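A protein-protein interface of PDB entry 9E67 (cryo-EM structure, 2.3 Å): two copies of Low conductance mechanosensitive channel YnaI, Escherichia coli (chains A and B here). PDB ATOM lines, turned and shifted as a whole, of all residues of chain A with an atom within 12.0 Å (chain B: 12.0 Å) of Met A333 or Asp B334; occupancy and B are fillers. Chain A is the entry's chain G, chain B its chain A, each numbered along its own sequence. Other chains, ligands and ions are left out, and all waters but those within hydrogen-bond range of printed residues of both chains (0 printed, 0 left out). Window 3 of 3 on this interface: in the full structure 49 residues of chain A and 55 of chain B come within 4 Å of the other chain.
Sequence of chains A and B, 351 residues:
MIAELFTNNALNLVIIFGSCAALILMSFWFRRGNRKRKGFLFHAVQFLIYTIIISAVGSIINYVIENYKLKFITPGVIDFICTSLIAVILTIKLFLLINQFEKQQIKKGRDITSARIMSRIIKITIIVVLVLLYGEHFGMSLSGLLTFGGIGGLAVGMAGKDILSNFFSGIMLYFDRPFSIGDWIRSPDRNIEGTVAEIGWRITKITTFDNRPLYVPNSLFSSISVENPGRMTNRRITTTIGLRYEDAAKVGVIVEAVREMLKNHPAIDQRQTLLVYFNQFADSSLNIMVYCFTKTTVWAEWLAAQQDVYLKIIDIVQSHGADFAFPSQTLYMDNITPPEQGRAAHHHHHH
The backbone carbonyl oxygen (O) of Tyr B332 lies within hydrogen-bond range of the backbone NH (N) of Leu A331 (2.9 Å). The backbone NH (N) of Asp B334 sits at hydrogen-bond distance from the backbone carbonyl oxygen (O) of Leu A331 (3.3 Å). The backbone NH (N) of Tyr B332 is in hydrogen-bond range of the backbone carbonyl oxygen (O) of Gln A329 (2.9 Å). O of Thr B330 sits at hydrogen-bond distance from N of Gln A329 (3.1 Å).
Ser A328 touches Thr B330. CB of Ser A328 touches CE2 of Tyr B332 (3.9 Å). Leu B331 touches Gln A329 (CA to O, 3.7 Å). Tyr B332 touches Thr A330 (O to CA, 3.5 Å). Leu A331 touches Leu B331 (CD1 to CD1, 3.9 Å). O of Leu A331 touches CA of Met B333, 3.9 Å away. Met A333 touches Met B333 (SD to CE, 3.5 Å). Met A333 touches Asp B334.
Of chain B, only Met B333 and Asp B334 come within 4 Å of Met A333. Asp B334 touches just these residues of chain A: Leu A331 and Met A333. Printed residues of chain B within 4 Å of Leu A331: Leu B331 (3.9 Å), Tyr B332 (2.9 Å), Met B333 (3.9 Å) and Asp B334 (3.3 Å). No residue of chain B comes within 4 Å of Tyr A332. Met B333 touches just these residues of chain A: Leu A331 and Met A333. Of the printed residues of chain B, Ser A328 touches Thr B330 (3.2 Å) and Tyr B332 (3.9 Å). Printed residues of chain A within 4 Å of Leu B331: Gln A329 and Leu A331. Of the printed residues of chain A, Thr B330 touches Ser A328 and Gln A329. The nearest residue of chain B that does not touch Met A333 is Tyr B332 (7.5 Å). The nearest residue of chain A that does not touch Asp B334 is Tyr A332 (4.1 Å).
Hydrophobic or aromatic side chains of chain A within 4 Å of the printed part of chain B: Leu A331 and Met A333. Among the printed residues, 12 pairs touch across the chains. Among the printed residues, no Asp or Glu carboxylate lies within 4 Å of a Lys or Arg side-chain nitrogen of the other chain.
Thr A330 touches Tyr B332, but with the chains exchanged Tyr A332 does not touch Thr B330 (10.9 Å). Leu A331 touches Asp B334, but with the chains exchanged Asp A334 does not touch Leu B331 (13.6 Å). Met B333 touches its own counterpart, Met A333. Met A333 touches Asp B334, but with the chains exchanged Asp A334 does not touch Met B333 (8.3 Å). Of the 12 pairs that touch across the chains among the printed residues, 2 have their exchanged pair printed and touching as well.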
ATOM      1  N   SER A 328       4.621  16.615  19.000  1.00  0.00           N
ATOM      2  CA  SER A 328       4.066  17.679  19.823  1.00  0.00           C
ATOM      3  C   SER A 328       4.426  17.473  21.287  1.00  0.00           C
ATOM      4  O   SER A 328       4.687  16.351  21.731  1.00  0.00           O
ATOM      5  CB  SER A 328       2.543  17.756  19.676  1.00  0.00           C
ATOM      6  OG  SER A 328       2.166  17.845  18.314  1.00  0.00           O
ATOM      7  N   GLN A 329       4.437  18.576  22.032  1.00  0.00           N
ATOM      8  CA  GLN A 329       4.788  18.557  23.442  1.00  0.00           C
ATOM      9  C   GLN A 329       4.027  19.655  24.166  1.00  0.00           C
ATOM     10  O   GLN A 329       3.761  20.721  23.604  1.00  0.00           O
ATOM     11  CB  GLN A 329       6.295  18.745  23.651  1.00  0.00           C
ATOM     12  CG  GLN A 329       7.115  17.486  23.468  1.00  0.00           C
ATOM     13  CD  GLN A 329       8.470  17.577  24.129  1.00  0.00           C
ATOM     14  OE1 GLN A 329       9.260  18.467  23.824  1.00  0.00           O
ATOM     15  NE2 GLN A 329       8.743  16.660  25.047  1.00  0.00           N
ATOM     16  N   THR A 330       3.682  19.386  25.420  1.00  0.00           N
ATOM     17  CA  THR A 330       3.120  20.387  26.316  1.00  0.00           C
ATOM     18  C   THR A 330       4.204  20.831  27.287  1.00  0.00           C
ATOM     19  O   THR A 330       4.827  19.996  27.949  1.00  0.00           O
ATOM     20  CB  THR A 330       1.917  19.834  27.081  1.00  0.00           C
ATOM     21  OG1 THR A 330       0.884  19.472  26.158  1.00  0.00           O
ATOM     22  CG2 THR A 330       1.373  20.876  28.043  1.00  0.00           C
ATOM     23  N   LEU A 331       4.433  22.137  27.365  1.00  0.00           N
ATOM     24  CA  LEU A 331       5.530  22.690  28.147  1.00  0.00           C
ATOM     25  C   LEU A 331       4.987  23.499  29.315  1.00  0.00           C
ATOM     26  O   LEU A 331       4.134  24.371  29.130  1.00  0.00           O
ATOM     27  CB  LEU A 331       6.432  23.565  27.275  1.00  0.00           C
ATOM     28  CG  LEU A 331       7.041  22.883  26.051  1.00  0.00           C
ATOM     29  CD1 LEU A 331       7.873  23.868  25.250  1.00  0.00           C
ATOM     30  CD2 LEU A 331       7.875  21.683  26.461  1.00  0.00           C
ATOM     31  N   TYR A 332       5.485  23.203  30.512  1.00  0.00           N
ATOM     32  CA  TYR A 332       5.155  23.946  31.722  1.00  0.00           C
ATOM     33  C   TYR A 332       6.394  24.707  32.166  1.00  0.00           C
ATOM     34  O   TYR A 332       7.447  24.104  32.392  1.00  0.00           O
ATOM     35  CB  TYR A 332       4.679  23.009  32.830  1.00  0.00           C
ATOM     36  CG  TYR A 332       3.472  22.181  32.464  1.00  0.00           C
ATOM     37  CD1 TYR A 332       2.187  22.670  32.649  1.00  0.00           C
ATOM     38  CD2 TYR A 332       3.617  20.905  31.938  1.00  0.00           C
ATOM     39  CE1 TYR A 332       1.084  21.912  32.317  1.00  0.00           C
ATOM     40  CE2 TYR A 332       2.521  20.143  31.604  1.00  0.00           C
ATOM     41  CZ  TYR A 332       1.258  20.650  31.794  1.00  0.00           C
ATOM     42  OH  TYR A 332       0.162  19.890  31.461  1.00  0.00           O
ATOM     43  N   MET A 333       6.271  26.022  32.291  1.00  0.00           N
ATOM     44  CA  MET A 333       7.385  26.870  32.685  1.00  0.00           C
ATOM     45  C   MET A 333       7.247  27.297  34.139  1.00  0.00           C
ATOM     46  O   MET A 333       6.142  27.389  34.680  1.00  0.00           O
ATOM     47  CB  MET A 333       7.477  28.104  31.787  1.00  0.00           C
ATOM     48  CG  MET A 333       6.991  27.865  30.372  1.00  0.00           C
ATOM     49  SD  MET A 333       8.330  27.388  29.266  1.00  0.00           S
ATOM     50  CE  MET A 333       9.475  28.737  29.527  1.00  0.00           C
ATOM     51  N   ASP A 334       8.390  27.548  34.770  1.00  0.00           N
ATOM     52  CA  ASP A 334       8.435  27.979  36.162  1.00  0.00           C
ATOM     53  C   ASP A 334       7.696  29.298  36.365  1.00  0.00           C
ATOM     54  O   ASP A 334       6.834  29.409  37.237  1.00  0.00           O
ATOM     55  CB  ASP A 334       9.885  28.115  36.625  1.00  0.00           C
ATOM     56  CG  ASP A 334      10.704  29.019  35.721  1.00  0.00           C
ATOM     57  OD1 ASP A 334      10.252  29.300  34.592  1.00  0.00           O
ATOM     58  OD2 ASP A 334      11.800  29.448  36.139  1.00  0.00           O
ATOM     59  N   THR B 330       5.744  20.857  17.362  1.00  0.00           N
ATOM     60  CA  THR B 330       4.687  21.784  17.738  1.00  0.00           C
ATOM     61  C   THR B 330       4.632  21.866  19.256  1.00  0.00           C
ATOM     62  O   THR B 330       4.535  20.838  19.933  1.00  0.00           O
ATOM     63  CB  THR B 330       3.333  21.335  17.181  1.00  0.00           C
ATOM     64  OG1 THR B 330       3.382  21.322  15.750  1.00  0.00           O
ATOM     65  CG2 THR B 330       2.234  22.283  17.627  1.00  0.00           C
ATOM     66  N   LEU B 331       4.704  23.081  19.789  1.00  0.00           N
ATOM     67  CA  LEU B 331       4.806  23.298  21.224  1.00  0.00           C
ATOM     68  C   LEU B 331       3.552  23.987  21.738  1.00  0.00           C
ATOM     69  O   LEU B 331       3.116  24.995  21.174  1.00  0.00           O
ATOM     70  CB  LEU B 331       6.042  24.132  21.563  1.00  0.00           C
ATOM     71  CG  LEU B 331       7.382  23.580  21.077  1.00  0.00           C
ATOM     72  CD1 LEU B 331       8.516  24.512  21.466  1.00  0.00           C
ATOM     73  CD2 LEU B 331       7.623  22.184  21.620  1.00  0.00           C
ATOM     74  N   TYR B 332       2.979  23.440  22.806  1.00  0.00           N
ATOM     75  CA  TYR B 332       1.827  24.026  23.479  1.00  0.00           C
ATOM     76  C   TYR B 332       2.275  24.532  24.841  1.00  0.00           C
ATOM     77  O   TYR B 332       2.809  23.761  25.647  1.00  0.00           O
ATOM     78  CB  TYR B 332       0.698  23.008  23.628  1.00  0.00           C
ATOM     79  CG  TYR B 332       0.202  22.447  22.318  1.00  0.00           C
ATOM     80  CD1 TYR B 332      -0.790  23.093  21.596  1.00  0.00           C
ATOM     81  CD2 TYR B 332       0.723  21.270  21.805  1.00  0.00           C
ATOM     82  CE1 TYR B 332      -1.245  22.584  20.401  1.00  0.00           C
ATOM     83  CE2 TYR B 332       0.275  20.754  20.611  1.00  0.00           C
ATOM     84  CZ  TYR B 332      -0.709  21.413  19.913  1.00  0.00           C
ATOM     85  OH  TYR B 332      -1.160  20.900  18.721  1.00  0.00           O
ATOM     86  N   MET B 333       2.058  25.815  25.098  1.00  0.00           N
ATOM     87  CA  MET B 333       2.497  26.451  26.328  1.00  0.00           C
ATOM     88  C   MET B 333       1.346  26.539  27.320  1.00  0.00           C
ATOM     89  O   MET B 333       0.177  26.630  26.940  1.00  0.00           O
ATOM     90  CB  MET B 333       3.052  27.848  26.046  1.00  0.00           C
ATOM     91  CG  MET B 333       3.996  27.900  24.857  1.00  0.00           C
ATOM     92  SD  MET B 333       5.669  27.376  25.267  1.00  0.00           S
ATOM     93  CE  MET B 333       5.889  28.207  26.836  1.00  0.00           C
ATOM     94  N   ASP B 334       1.694  26.501  28.604  1.00  0.00           N
ATOM     95  CA  ASP B 334       0.707  26.578  29.676  1.00  0.00           C
ATOM     96  C   ASP B 334      -0.031  27.913  29.662  1.00  0.00           C
ATOM     97  O   ASP B 334      -1.260  27.954  29.591  1.00  0.00           O
ATOM     98  CB  ASP B 334       1.382  26.366  31.032  1.00  0.00           C
ATOM     99  CG  ASP B 334       2.539  27.317  31.262  1.00  0.00           C
ATOM    100  OD1 ASP B 334       3.012  27.932  30.282  1.00  0.00           O
ATOM    101  OD2 ASP B 334       2.981  27.454  32.422  1.00  0.00           O
